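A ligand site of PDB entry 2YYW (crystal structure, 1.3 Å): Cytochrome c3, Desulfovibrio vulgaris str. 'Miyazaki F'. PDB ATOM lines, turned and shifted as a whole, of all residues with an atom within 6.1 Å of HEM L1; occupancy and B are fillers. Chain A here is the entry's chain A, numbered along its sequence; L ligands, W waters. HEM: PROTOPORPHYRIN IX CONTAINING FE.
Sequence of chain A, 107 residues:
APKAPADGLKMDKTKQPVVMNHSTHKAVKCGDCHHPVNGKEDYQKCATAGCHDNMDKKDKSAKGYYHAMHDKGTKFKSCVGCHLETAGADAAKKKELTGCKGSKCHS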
ATOM      1  N   MET A  11      18.687 -16.906 -12.182  1.00  0.00           N
ATOM      2  CA  MET A  11      19.313 -16.918 -13.500  1.00  0.00           C
ATOM      3  C   MET A  11      20.609 -17.696 -13.263  1.00  0.00           C
ATOM      4  O   MET A  11      21.492 -17.182 -12.547  1.00  0.00           O
ATOM      5  CB  MET A  11      19.533 -15.491 -13.991  1.00  0.00           C
ATOM      6  CG  MET A  11      18.158 -14.744 -14.089  1.00  0.00           C
ATOM      7  SD  MET A  11      18.442 -13.019 -14.618  1.00  0.00           S
ATOM      8  CE  MET A  11      18.732 -13.279 -16.386  1.00  0.00           C
ATOM      9  N   ASP A  12      20.683 -18.896 -13.823  1.00  0.00           N
ATOM     10  CA  ASP A  12      21.819 -19.779 -13.495  1.00  0.00           C
ATOM     11  C   ASP A  12      22.354 -20.509 -14.710  1.00  0.00           C
ATOM     12  O   ASP A  12      22.711 -21.679 -14.620  1.00  0.00           O
ATOM     13  CB  ASP A  12      21.460 -20.749 -12.377  1.00  0.00           C
ATOM     14  CG  ASP A  12      20.234 -21.562 -12.721  1.00  0.00           C
ATOM     15  OD1 ASP A  12      19.843 -21.647 -13.922  1.00  0.00           O
ATOM     16  OD2 ASP A  12      19.712 -22.121 -11.730  1.00  0.00           O
ATOM     17  N   LYS A  13      22.539 -19.758 -15.795  1.00  0.00           N
ATOM     18  CA  LYS A  13      23.200 -20.330 -16.971  1.00  0.00           C
ATOM     19  C   LYS A  13      24.721 -20.363 -16.782  1.00  0.00           C
ATOM     20  O   LYS A  13      25.405 -21.045 -17.549  1.00  0.00           O
ATOM     21  CB  LYS A  13      22.905 -19.517 -18.236  1.00  0.00           C
ATOM     22  CG  LYS A  13      21.430 -19.299 -18.511  1.00  0.00           C
ATOM     23  CD  LYS A  13      20.610 -20.554 -18.615  1.00  0.00           C
ATOM     24  CE  LYS A  13      20.928 -21.375 -19.824  1.00  0.00           C
ATOM     25  NZ  LYS A  13      19.953 -22.508 -19.882  1.00  0.00           N
ATOM     26  N   THR A  14      25.203 -19.604 -15.816  1.00  0.00           N
ATOM     27  CA  THR A  14      26.640 -19.432 -15.622  1.00  0.00           C
ATOM     28  C   THR A  14      27.048 -19.814 -14.204  1.00  0.00           C
ATOM     29  O   THR A  14      26.207 -20.126 -13.360  1.00  0.00           O
ATOM     30  CB  THR A  14      27.090 -17.991 -15.873  1.00  0.00           C
ATOM     31  OG1 THR A  14      26.835 -17.161 -14.724  1.00  0.00           O
ATOM     32  CG2 THR A  14      26.345 -17.359 -17.069  1.00  0.00           C
ATOM     33  N   LYS A  15      28.360 -19.756 -13.917  1.00  0.00           N
ATOM     34  CA  LYS A  15      28.876 -20.022 -12.587  1.00  0.00           C
ATOM     35  C   LYS A  15      28.767 -18.799 -11.685  1.00  0.00           C
ATOM     36  O   LYS A  15      29.192 -18.849 -10.513  1.00  0.00           O
ATOM     37  CB  LYS A  15      30.313 -20.547 -12.685  1.00  0.00           C
ATOM     38  CG  LYS A  15      30.339 -21.979 -13.249  1.00  0.00           C
ATOM     39  CD  LYS A  15      31.767 -22.494 -13.220  1.00  0.00           C
ATOM     40  CE  LYS A  15      31.867 -23.743 -14.085  1.00  0.00           C
ATOM     41  NZ  LYS A  15      33.260 -24.244 -14.101  1.00  0.00           N
ATOM     42  N   GLN A  16      28.145 -17.703 -12.162  1.00  0.00           N
ATOM     43  CA  GLN A  16      27.887 -16.524 -11.342  1.00  0.00           C
ATOM     44  C   GLN A  16      26.368 -16.231 -11.359  1.00  0.00           C
ATOM     45  O   GLN A  16      25.919 -15.220 -11.895  1.00  0.00           O
ATOM     46  CB  GLN A  16      28.667 -15.285 -11.803  1.00  0.00           C
ATOM     47  CG  GLN A  16      30.141 -15.550 -12.081  1.00  0.00           C
ATOM     48  CD  GLN A  16      30.966 -15.925 -10.878  1.00  0.00           C
ATOM     49  OE1 GLN A  16      30.537 -15.699  -9.757  1.00  0.00           O
ATOM     50  NE2 GLN A  16      32.150 -16.458 -11.116  1.00  0.00           N
ATOM     51  N   PRO A  17      25.555 -17.118 -10.765  1.00  0.00           N
ATOM     52  CA  PRO A  17      24.097 -16.978 -10.867  1.00  0.00           C
ATOM     53  C   PRO A  17      23.574 -15.741 -10.134  1.00  0.00           C
ATOM     54  O   PRO A  17      24.178 -15.256  -9.153  1.00  0.00           O
ATOM     55  CB  PRO A  17      23.548 -18.225 -10.156  1.00  0.00           C
ATOM     56  CG  PRO A  17      24.672 -18.724  -9.340  1.00  0.00           C
ATOM     57  CD  PRO A  17      25.948 -18.313  -9.996  1.00  0.00           C
ATOM     58  N   VAL A  18      22.442 -15.230 -10.586  1.00  0.00           N
ATOM     59  CA  VAL A  18      21.874 -13.956 -10.105  1.00  0.00           C
ATOM     60  C   VAL A  18      20.394 -14.133  -9.885  1.00  0.00           C
ATOM     61  O   VAL A  18      19.750 -14.827 -10.683  1.00  0.00           O
ATOM     62  CB  VAL A  18      22.157 -12.819 -11.132  1.00  0.00           C
ATOM     63  CG1 VAL A  18      21.484 -11.511 -10.763  1.00  0.00           C
ATOM     64  CG2 VAL A  18      23.665 -12.634 -11.243  1.00  0.00           C
ATOM     65  N   MET A  55      27.184 -18.435 -24.860  1.00  0.00           N
ATOM     66  CA  MET A  55      27.720 -18.342 -23.494  1.00  0.00           C
ATOM     67  C   MET A  55      29.169 -17.936 -23.504  1.00  0.00           C
ATOM     68  O   MET A  55      29.824 -18.076 -22.444  1.00  0.00           O
ATOM     69  CB  MET A  55      27.489 -19.668 -22.741  1.00  0.00           C
ATOM     70  CG  MET A  55      25.981 -19.907 -22.527  1.00  0.00           C
ATOM     71  SD  MET A  55      25.323 -18.718 -21.312  1.00  0.00           S
ATOM     72  CE  MET A  55      23.593 -18.719 -21.843  1.00  0.00           C
ATOM     73  N   ASP A  56      29.675 -17.414 -24.600  1.00  0.00           N
ATOM     74  CA  ASP A  56      30.991 -16.776 -24.611  1.00  0.00           C
ATOM     75  C   ASP A  56      30.828 -15.317 -24.140  1.00  0.00           C
ATOM     76  O   ASP A  56      30.186 -14.513 -24.810  1.00  0.00           O
ATOM     77  CB  ASP A  56      31.669 -16.782 -25.962  1.00  0.00           C
ATOM     78  CG  ASP A  56      33.066 -16.179 -25.836  1.00  0.00           C
ATOM     79  OD1 ASP A  56      33.243 -14.998 -25.664  1.00  0.00           O
ATOM     80  OD2 ASP A  56      34.122 -16.891 -25.848  1.00  0.00           O
ATOM     81  N   LYS A  57      31.383 -14.998 -22.976  1.00  0.00           N
ATOM     82  CA  LYS A  57      31.104 -13.696 -22.348  1.00  0.00           C
ATOM     83  C   LYS A  57      31.751 -12.532 -23.081  1.00  0.00           C
ATOM     84  O   LYS A  57      31.473 -11.385 -22.680  1.00  0.00           O
ATOM     85  CB  LYS A  57      31.486 -13.748 -20.860  1.00  0.00           C
ATOM     86  CG  LYS A  57      32.998 -13.797 -20.590  1.00  0.00           C
ATOM     87  CD  LYS A  57      33.213 -13.827 -19.058  1.00  0.00           C
ATOM     88  CE  LYS A  57      34.649 -14.251 -18.761  1.00  0.00           C
ATOM     89  NZ  LYS A  57      34.874 -14.261 -17.287  1.00  0.00           N
ATOM     90  N   TYR A  65      24.825 -13.772 -24.344  1.00  0.00           N
ATOM     91  CA  TYR A  65      24.086 -13.717 -23.078  1.00  0.00           C
ATOM     92  C   TYR A  65      24.692 -12.691 -22.096  1.00  0.00           C
ATOM     93  O   TYR A  65      23.984 -11.833 -21.551  1.00  0.00           O
ATOM     94  CB  TYR A  65      24.077 -15.108 -22.470  1.00  0.00           C
ATOM     95  CG  TYR A  65      23.303 -15.281 -21.181  1.00  0.00           C
ATOM     96  CD1 TYR A  65      23.971 -15.426 -19.955  1.00  0.00           C
ATOM     97  CD2 TYR A  65      21.927 -15.304 -21.146  1.00  0.00           C
ATOM     98  CE1 TYR A  65      23.278 -15.586 -18.774  1.00  0.00           C
ATOM     99  CE2 TYR A  65      21.229 -15.483 -19.979  1.00  0.00           C
ATOM    100  CZ  TYR A  65      21.900 -15.633 -18.784  1.00  0.00           C
ATOM    101  OH  TYR A  65      21.154 -15.787 -17.623  1.00  0.00           O
ATOM    102  N   TYR A  66      26.011 -12.789 -21.894  1.00  0.00           N
ATOM    103  CA  TYR A  66      26.682 -11.813 -21.021  1.00  0.00           C
ATOM    104  C   TYR A  66      26.377 -10.402 -21.534  1.00  0.00           C
ATOM    105  O   TYR A  66      26.081  -9.502 -20.740  1.00  0.00           O
ATOM    106  CB  TYR A  66      28.191 -12.089 -20.952  1.00  0.00           C
ATOM    107  CG  TYR A  66      28.950 -11.097 -20.086  1.00  0.00           C
ATOM    108  CD1 TYR A  66      29.385  -9.827 -20.528  1.00  0.00           C
ATOM    109  CD2 TYR A  66      29.260 -11.397 -18.764  1.00  0.00           C
ATOM    110  CE1 TYR A  66      30.057  -8.943 -19.726  1.00  0.00           C
ATOM    111  CE2 TYR A  66      29.943 -10.533 -17.916  1.00  0.00           C
ATOM    112  CZ  TYR A  66      30.332  -9.316 -18.434  1.00  0.00           C
ATOM    113  OH  TYR A  66      31.013  -8.448 -17.618  1.00  0.00           O
ATOM    114  N   MET A  69      23.146  -8.770 -20.539  1.00  0.00           N
ATOM    115  CA  MET A  69      22.938  -8.477 -19.135  1.00  0.00           C
ATOM    116  C   MET A  69      23.827  -7.309 -18.678  1.00  0.00           C
ATOM    117  O   MET A  69      23.474  -6.690 -17.680  1.00  0.00           O
ATOM    118  CB  MET A  69      23.197  -9.674 -18.193  1.00  0.00           C
ATOM    119  CG  MET A  69      22.425 -10.926 -18.622  1.00  0.00           C
ATOM    120  SD  MET A  69      20.639 -10.663 -18.766  1.00  0.00           S
ATOM    121  CE  MET A  69      20.145 -12.122 -19.652  1.00  0.00           C
ATOM    122  N   HIS A  70      24.942  -7.046 -19.376  1.00  0.00           N
ATOM    123  CA  HIS A  70      25.959  -6.145 -18.836  1.00  0.00           C
ATOM    124  C   HIS A  70      26.244  -4.882 -19.649  1.00  0.00           C
ATOM    125  O   HIS A  70      26.823  -3.962 -19.051  1.00  0.00           O
ATOM    126  CB  HIS A  70      27.311  -6.906 -18.662  1.00  0.00           C
ATOM    127  CG  HIS A  70      27.225  -8.007 -17.642  1.00  0.00           C
ATOM    128  ND1 HIS A  70      26.800  -9.293 -17.993  1.00  0.00           N
ATOM    129  CD2 HIS A  70      27.510  -8.055 -16.321  1.00  0.00           C
ATOM    130  CE1 HIS A  70      26.828 -10.054 -16.892  1.00  0.00           C
ATOM    131  NE2 HIS A  70      27.249  -9.331 -15.876  1.00  0.00           N
ATOM    132  N   CYS A  79      20.622  -5.140 -17.728  1.00  0.00           N
ATOM    133  CA  CYS A  79      20.588  -5.035 -16.281  1.00  0.00           C
ATOM    134  C   CYS A  79      21.536  -3.927 -15.838  1.00  0.00           C
ATOM    135  O   CYS A  79      21.138  -2.982 -15.123  1.00  0.00           O
ATOM    136  CB  CYS A  79      21.039  -6.328 -15.573  1.00  0.00           C
ATOM    137  SG  CYS A  79      20.374  -7.906 -16.223  1.00  0.00           S
ATOM    138  N   VAL A  80      22.795  -4.032 -16.262  1.00  0.00           N
ATOM    139  CA  VAL A  80      23.792  -3.054 -15.767  1.00  0.00           C
ATOM    140  C   VAL A  80      23.518  -1.691 -16.380  1.00  0.00           C
ATOM    141  O   VAL A  80      23.671  -0.680 -15.672  1.00  0.00           O
ATOM    142  CB  VAL A  80      25.215  -3.537 -16.039  1.00  0.00           C
ATOM    143  CG1 VAL A  80      26.238  -2.466 -15.624  1.00  0.00           C
ATOM    144  CG2 VAL A  80      25.507  -4.843 -15.297  1.00  0.00           C
ATOM    145  N   HIS A  83      20.710  -0.037 -14.564  1.00  0.00           N
ATOM    146  CA  HIS A  83      21.129   0.272 -13.206  1.00  0.00           C
ATOM    147  C   HIS A  83      22.092   1.416 -13.173  1.00  0.00           C
ATOM    148  O   HIS A  83      22.087   2.201 -12.178  1.00  0.00           O
ATOM    149  CB  HIS A  83      21.745  -0.970 -12.559  1.00  0.00           C
ATOM    150  CG  HIS A  83      20.712  -1.997 -12.168  1.00  0.00           C
ATOM    151  ND1 HIS A  83      21.077  -3.015 -11.311  1.00  0.00           N
ATOM    152  CD2 HIS A  83      19.410  -2.208 -12.430  1.00  0.00           C
ATOM    153  CE1 HIS A  83      20.026  -3.786 -11.100  1.00  0.00           C
ATOM    154  NE2 HIS A  83      18.988  -3.339 -11.758  1.00  0.00           N
ATOM    155  N   GLU A  96      25.964  -0.978  -5.141  1.00  0.00           N
ATOM    156  CA  GLU A  96      24.856  -1.896  -4.922  1.00  0.00           C
ATOM    157  C   GLU A  96      24.287  -2.436  -6.216  1.00  0.00           C
ATOM    158  O   GLU A  96      23.944  -3.631  -6.335  1.00  0.00           O
ATOM    159  CB  GLU A  96      23.712  -1.174  -4.211  1.00  0.00           C
ATOM    160  CG  GLU A  96      22.651  -1.883  -3.452  1.00  0.00           C
ATOM    161  CD  GLU A  96      21.785  -0.849  -2.717  1.00  0.00           C
ATOM    162  OE1 GLU A  96      20.678  -0.599  -3.212  1.00  0.00           O
ATOM    163  OE2 GLU A  96      22.253  -0.294  -1.697  1.00  0.00           O
ATOM    164  N   LEU A  97      24.123  -1.548  -7.200  1.00  0.00           N
ATOM    165  CA  LEU A  97      23.355  -1.912  -8.396  1.00  0.00           C
ATOM    166  C   LEU A  97      24.238  -2.250  -9.586  1.00  0.00           C
ATOM    167  O   LEU A  97      23.719  -2.866 -10.534  1.00  0.00           O
ATOM    168  CB  LEU A  97      22.434  -0.770  -8.771  1.00  0.00           C
ATOM    169  CG  LEU A  97      21.377  -0.396  -7.732  1.00  0.00           C
ATOM    170  CD1 LEU A  97      20.549   0.794  -8.218  1.00  0.00           C
ATOM    171  CD2 LEU A  97      20.471  -1.574  -7.422  1.00  0.00           C
ATOM    172  N   THR A  98      25.508  -1.816  -9.598  1.00  0.00           N
ATOM    173  CA  THR A  98      26.379  -2.078 -10.754  1.00  0.00           C
ATOM    174  C   THR A  98      27.712  -2.699 -10.405  1.00  0.00           C
ATOM    175  O   THR A  98      28.465  -3.004 -11.341  1.00  0.00           O
ATOM    176  CB  THR A  98      26.601  -0.820 -11.602  1.00  0.00           C
ATOM    177  OG1 THR A  98      27.497   0.110 -10.914  1.00  0.00           O
ATOM    178  CG2 THR A  98      25.281  -0.149 -11.889  1.00  0.00           C
ATOM    179  N   GLY A  99      28.014  -2.937  -9.124  1.00  0.00           N
ATOM    180  CA  GLY A  99      29.305  -3.485  -8.763  1.00  0.00           C
ATOM    181  C   GLY A  99      29.466  -4.890  -9.273  1.00  0.00           C
ATOM    182  O   GLY A  99      28.534  -5.720  -9.333  1.00  0.00           O
ATOM    183  N   CYS A 100      30.696  -5.231  -9.673  1.00  0.00           N
ATOM    184  CA  CYS A 100      30.917  -6.563 -10.240  1.00  0.00           C
ATOM    185  C   CYS A 100      31.047  -7.609  -9.153  1.00  0.00           C
ATOM    186  O   CYS A 100      30.885  -8.801  -9.427  1.00  0.00           O
ATOM    187  CB  CYS A 100      32.226  -6.546 -11.043  1.00  0.00           C
ATOM    188  SG  CYS A 100      32.264  -5.289 -12.350  1.00  0.00           S
ATOM    189  N   LYS A 101      31.356  -7.162  -7.945  1.00  0.00           N
ATOM    190  CA  LYS A 101      31.351  -8.041  -6.790  1.00  0.00           C
ATOM    191  C   LYS A 101      30.808  -7.235  -5.614  1.00  0.00           C
ATOM    192  O   LYS A 101      30.811  -5.996  -5.667  1.00  0.00           O
ATOM    193  CB  LYS A 101      32.744  -8.626  -6.490  1.00  0.00           C
ATOM    194  CG  LYS A 101      33.736  -7.548  -6.053  1.00  0.00           C
ATOM    195  CD  LYS A 101      35.127  -8.153  -5.831  1.00  0.00           C
ATOM    196  CE  LYS A 101      35.941  -7.294  -4.889  1.00  0.00           C
ATOM    197  NZ  LYS A 101      35.460  -7.422  -3.495  1.00  0.00           N
ATOM    198  N   SER A 103      27.812  -6.764  -4.867  1.00  0.00           N
ATOM    199  CA  SER A 103      26.630  -5.990  -5.286  1.00  0.00           C
ATOM    200  C   SER A 103      25.369  -6.805  -5.053  1.00  0.00           C
ATOM    201  O   SER A 103      25.406  -7.980  -4.625  1.00  0.00           O
ATOM    202  CB  SER A 103      26.757  -5.614  -6.755  1.00  0.00           C
ATOM    203  OG  SER A 103      26.646  -6.773  -7.577  1.00  0.00           O
ATOM    204  N   LYS A 104      24.209  -6.236  -5.372  1.00  0.00           N
ATOM    205  CA  LYS A 104      22.979  -7.003  -5.209  1.00  0.00           C
ATOM    206  C   LYS A 104      22.878  -8.062  -6.309  1.00  0.00           C
ATOM    207  O   LYS A 104      22.070  -8.966  -6.155  1.00  0.00           O
ATOM    208  CB  LYS A 104      21.773  -6.073  -5.195  1.00  0.00           C
ATOM    209  CG  LYS A 104      21.720  -5.113  -4.000  1.00  0.00           C
ATOM    210  CD  LYS A 104      20.306  -4.664  -3.685  1.00  0.00           C
ATOM    211  CE  LYS A 104      20.190  -3.819  -2.438  1.00  0.00           C
ATOM    212  NZ  LYS A 104      20.327  -4.605  -1.188  1.00  0.00           N
ATOM    213  N   CYS A 105      23.642  -8.003  -7.385  1.00  0.00           N
ATOM    214  CA  CYS A 105      23.669  -9.068  -8.382  1.00  0.00           C
ATOM    215  C   CYS A 105      24.690 -10.174  -8.020  1.00  0.00           C
ATOM    216  O   CYS A 105      24.337 -11.343  -8.044  1.00  0.00           O
ATOM    217  CB  CYS A 105      23.963  -8.552  -9.809  1.00  0.00           C
ATOM    218  SG  CYS A 105      22.654  -7.395 -10.257  1.00  0.00           S
ATOM    219  N   HIS A 106      25.925  -9.813  -7.718  1.00  0.00           N
ATOM    220  CA  HIS A 106      26.979 -10.733  -7.446  1.00  0.00           C
ATOM    221  C   HIS A 106      27.596 -10.535  -6.063  1.00  0.00           C
ATOM    222  O   HIS A 106      28.093  -9.463  -5.765  1.00  0.00           O
ATOM    223  CB  HIS A 106      28.106 -10.536  -8.478  1.00  0.00           C
ATOM    224  CG  HIS A 106      27.747 -10.790  -9.916  1.00  0.00           C
ATOM    225  ND1 HIS A 106      27.274 -11.982 -10.375  1.00  0.00           N
ATOM    226  CD2 HIS A 106      27.870 -10.017 -11.034  1.00  0.00           C
ATOM    227  CE1 HIS A 106      27.077 -11.918 -11.704  1.00  0.00           C
ATOM    228  NE2 HIS A 106      27.439 -10.729 -12.138  1.00  0.00           N
HETATM  229  CHA HEM L   1      26.866 -13.275 -15.075  1.00  0.00           C
HETATM  230  CHB HEM L   1      30.729 -10.447 -14.401  1.00  0.00           C
HETATM  231  CHC HEM L   1      27.923  -6.935 -12.751  1.00  0.00           C
HETATM  232  CHD HEM L   1      24.002  -9.564 -13.776  1.00  0.00           C
HETATM  233  C1A HEM L   1      28.190 -12.872 -14.896  1.00  0.00           C
HETATM  234  C2A HEM L   1      29.309 -13.623 -15.188  1.00  0.00           C
HETATM  235  C3A HEM L   1      30.425 -12.841 -15.007  1.00  0.00           C
HETATM  236  C4A HEM L   1      29.927 -11.597 -14.619  1.00  0.00           C
HETATM  237  CMA HEM L   1      31.895 -13.179 -15.195  1.00  0.00           C
HETATM  238  CAA HEM L   1      29.361 -15.057 -15.678  1.00  0.00           C
HETATM  239  CBA HEM L   1      29.618 -15.056 -17.202  1.00  0.00           C
HETATM  240  CGA HEM L   1      29.940 -16.451 -17.713  1.00  0.00           C
HETATM  241  O1A HEM L   1      30.816 -17.157 -17.128  1.00  0.00           O
HETATM  242  O2A HEM L   1      29.272 -16.928 -18.665  1.00  0.00           O
HETATM  243  C1B HEM L   1      30.299  -9.156 -14.036  1.00  0.00           C
HETATM  244  C2B HEM L   1      31.105  -8.033 -13.959  1.00  0.00           C
HETATM  245  C3B HEM L   1      30.338  -6.997 -13.444  1.00  0.00           C
HETATM  246  C4B HEM L   1      29.057  -7.561 -13.285  1.00  0.00           C
HETATM  247  CMB HEM L   1      32.580  -8.051 -14.346  1.00  0.00           C
HETATM  248  CAB HEM L   1      30.641  -5.599 -13.260  1.00  0.00           C
HETATM  249  CBB HEM L   1      30.778  -4.778 -14.498  1.00  0.00           C
HETATM  250  C1C HEM L   1      26.604  -7.421 -12.687  1.00  0.00           C
HETATM  251  C2C HEM L   1      25.523  -6.746 -12.117  1.00  0.00           C
HETATM  252  C3C HEM L   1      24.371  -7.473 -12.448  1.00  0.00           C
HETATM  253  C4C HEM L   1      24.828  -8.574 -13.206  1.00  0.00           C
HETATM  254  CMC HEM L   1      25.616  -5.472 -11.293  1.00  0.00           C
HETATM  255  CAC HEM L   1      23.003  -7.201 -12.107  1.00  0.00           C
HETATM  256  CBC HEM L   1      22.432  -5.859 -12.460  1.00  0.00           C
HETATM  257  C1D HEM L   1      24.447 -10.776 -14.354  1.00  0.00           C
HETATM  258  C2D HEM L   1      23.602 -11.806 -14.805  1.00  0.00           C
HETATM  259  C3D HEM L   1      24.416 -12.880 -15.132  1.00  0.00           C
HETATM  260  C4D HEM L   1      25.715 -12.477 -14.867  1.00  0.00           C
HETATM  261  CMD HEM L   1      22.070 -11.678 -14.936  1.00  0.00           C
HETATM  262  CAD HEM L   1      23.968 -14.236 -15.606  1.00  0.00           C
HETATM  263  CBD HEM L   1      23.501 -15.121 -14.479  1.00  0.00           C
HETATM  264  CGD HEM L   1      23.391 -16.582 -14.873  1.00  0.00           C
HETATM  265  O1D HEM L   1      22.505 -16.874 -15.733  1.00  0.00           O
HETATM  266  O2D HEM L   1      24.165 -17.427 -14.381  1.00  0.00           O
HETATM  267  NA  HEM L   1      28.577 -11.623 -14.574  1.00  0.00           N
HETATM  268  NB  HEM L   1      29.040  -8.859 -13.673  1.00  0.00           N
HETATM  269  NC  HEM L   1      26.161  -8.535 -13.300  1.00  0.00           N
HETATM  270  ND  HEM L   1      25.721 -11.218 -14.379  1.00  0.00           N
HETATM  271 FE   HEM L   1      27.374 -10.048 -13.992  1.00  0.00          FE
HETATM  272  CHA HEM L   2      16.911  -3.190  -8.572  1.00  0.00           C
HETATM  273  CHB HEM L   2      18.717  -7.071 -10.746  1.00  0.00           C
HETATM  274  CHC HEM L   2      17.354  -5.288 -15.005  1.00  0.00           C
HETATM  275  CHD HEM L   2      15.823  -1.275 -12.854  1.00  0.00           C
HETATM  276  C1A HEM L   2      17.514  -4.449  -8.760  1.00  0.00           C
HETATM  277  C2A HEM L   2      18.030  -5.232  -7.729  1.00  0.00           C
HETATM  278  C3A HEM L   2      18.588  -6.327  -8.351  1.00  0.00           C
HETATM  279  C4A HEM L   2      18.320  -6.197  -9.713  1.00  0.00           C
HETATM  280  CMA HEM L   2      19.327  -7.532  -7.793  1.00  0.00           C
HETATM  281  CAA HEM L   2      17.964  -4.979  -6.251  1.00  0.00           C
HETATM  282  CBA HEM L   2      16.605  -5.354  -5.666  1.00  0.00           C
HETATM  283  CGA HEM L   2      16.449  -6.860  -5.812  1.00  0.00           C
HETATM  284  O1A HEM L   2      17.123  -7.582  -5.059  1.00  0.00           O
HETATM  285  O2A HEM L   2      15.588  -7.314  -6.568  1.00  0.00           O
HETATM  286  C1B HEM L   2      18.475  -6.949 -12.120  1.00  0.00           C
HETATM  287  C2B HEM L   2      18.876  -7.886 -13.103  1.00  0.00           C
HETATM  288  C3B HEM L   2      18.478  -7.363 -14.323  1.00  0.00           C
HETATM  289  C4B HEM L   2      17.783  -6.179 -14.037  1.00  0.00           C
HETATM  290  CMB HEM L   2      19.576  -9.172 -12.771  1.00  0.00           C
HETATM  291  CAB HEM L   2      18.600  -7.936 -15.644  1.00  0.00           C
HETATM  292  CBB HEM L   2      18.082  -9.297 -15.832  1.00  0.00           C
HETATM  293  C1C HEM L   2      16.911  -3.956 -14.815  1.00  0.00           C
HETATM  294  C2C HEM L   2      16.538  -3.090 -15.859  1.00  0.00           C
HETATM  295  C3C HEM L   2      16.116  -1.881 -15.261  1.00  0.00           C
HETATM  296  C4C HEM L   2      16.234  -2.137 -13.881  1.00  0.00           C
HETATM  297  CMC HEM L   2      16.633  -3.488 -17.337  1.00  0.00           C
HETATM  298  CAC HEM L   2      15.680  -0.671 -15.873  1.00  0.00           C
HETATM  299  CBC HEM L   2      15.068  -0.625 -17.214  1.00  0.00           C
HETATM  300  C1D HEM L   2      16.001  -1.430 -11.464  1.00  0.00           C
HETATM  301  C2D HEM L   2      15.497  -0.540 -10.504  1.00  0.00           C
HETATM  302  C3D HEM L   2      15.780  -1.127  -9.279  1.00  0.00           C
HETATM  303  C4D HEM L   2      16.445  -2.303  -9.544  1.00  0.00           C
HETATM  304  CMD HEM L   2      14.837   0.792 -10.827  1.00  0.00           C
HETATM  305  CAD HEM L   2      15.614  -0.467  -7.937  1.00  0.00           C
HETATM  306  CBD HEM L   2      16.830   0.300  -7.481  1.00  0.00           C
HETATM  307  CGD HEM L   2      17.014   0.418  -5.982  1.00  0.00           C
HETATM  308  O1D HEM L   2      17.854   1.240  -5.581  1.00  0.00           O
HETATM  309  O2D HEM L   2      15.918   0.476  -5.358  1.00  0.00           O
HETATM  310  NA  HEM L   2      17.668  -5.046  -9.951  1.00  0.00           N
HETATM  311  NB  HEM L   2      17.930  -5.902 -12.733  1.00  0.00           N
HETATM  312  NC  HEM L   2      16.751  -3.351 -13.625  1.00  0.00           N
HETATM  313  ND  HEM L   2      16.458  -2.549 -10.859  1.00  0.00           N
HETATM  314 FE   HEM L   2      17.187  -4.208 -11.781  1.00  0.00          FE
HETATM  315  O   HOH W   1      33.227 -16.419 -16.363  1.00  0.00           O
HETATM  316  O   HOH W   2      29.232 -19.177 -20.007  1.00  0.00           O
HETATM  317  O   HOH W   3      30.414 -19.439 -15.914  1.00  0.00           O
HETATM  318  O   HOH W   4      27.457 -16.075 -20.441  1.00  0.00           O
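A carbon (CAB) of HEM L1 is bonded to the side-chain sulfur of Cys 100 (1.9 Å).
A carbon (CAC) of HEM L1 is bonded to the side-chain sulfur (SG) of Cys 105, 1.9 Å away.
An iron atom (FE) of HEM L1 is bound by a ring nitrogen (NE2) of His 106 (2.0 Å).
An iron atom (FE) of HEM L1 is bound by a ring nitrogen (NE2) of His 70, 2.0 Å away.
O1D of HEM L1 sits at hydrogen-bond distance from OH of Tyr 65, at 2.6 Å.
The backbone NH of Thr 14 is in hydrogen-bond range of an oxygen (O2D) of HEM L1.
The side-chain hydroxyl (OG1) of Thr 14 is in hydrogen-bond range of an oxygen (O2D) of HEM L1.
N of Lys 13 lies within hydrogen-bond range of O1D of HEM L1 (2.9 Å).
The backbone NH (N) of Asp 12 lies within hydrogen-bond range of an oxygen (O1D) of HEM L1.
An iron atom (FE) of HEM L2 is bound by a ring nitrogen (NE2) of His 83 (2.0 Å).
SG of Cys 79 is bonded to CAB of HEM L2 (1.9 Å).
The backbone NH of Cys 105 sits close to the side-chain hydroxyl of Ser 103 (3.3 Å).
OG of Ser 103 sits at hydrogen-bond distance from N of His 106, 3.1 Å away.
A ring nitrogen (ND1) of His 70 lies within hydrogen-bond range of the backbone carbonyl oxygen (O) of Tyr 66, at 2.8 Å.
The backbone NH (N) of Met 11 is in hydrogen-bond range of the backbone carbonyl oxygen (O) of Val 18 (2.8 Å).
O of Leu 97 sits at hydrogen-bond distance from ND1 of His 83, at 2.8 Å.
The backbone NH of Cys 79 lies close to the backbone carbonyl oxygen of Met 69 (3.2 Å).
The backbone carbonyl oxygen of Gly 99 lies within hydrogen-bond range of the side-chain hydroxyl of Ser 103.
O of Met 69 sits at hydrogen-bond distance from N of Val 80 (3.1 Å).
The backbone carbonyl oxygen of Met 11 lies close to an oxygen (O2D) of HEM L1, at 3.3 Å.
Residues that only touch HEM L1: Leu 97 (3.3 Å), His 83 (3.4 Å), Cys 79 (3.4 Å), Tyr 66 (3.5 Å), Thr 98 (3.5 Å), Gly 99 (3.5 Å), Gln 16 (3.5 Å), Pro 17 (3.5 Å), Val 18 (3.7 Å), Val 80 (3.7 Å), Met 69 (3.8 Å), Lys 57 (3.8 Å) and Met 55 (3.99 Å).
22 residues have an atom within 4 Å of HEM L1: Met 11, Asp 12, Lys 13, Thr 14, Gln 16, Pro 17, Val 18, Met 55, Lys 57, Tyr 65, Tyr 66, Met 69, His 70, Cys 79, Val 80, His 83, Leu 97, Thr 98, Gly 99, Cys 100, Cys 105 and His 106.
Water W3 bridges O1A of HEM L1 and N of Lys 15.
Water W2 lies within hydrogen-bond range of O2A of HEM L1 (2.6 Å) and O of Met 55 (2.7 Å).
Water W1 lies within hydrogen-bond range of an oxygen (O1A) of HEM L1 (2.6 Å) and the side-chain amino group (NZ) of Lys 57 (2.9 Å).
Water W4 bridges O2A of HEM L1 (2.7 Å) and SD of Met 55 (3.5 Å).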
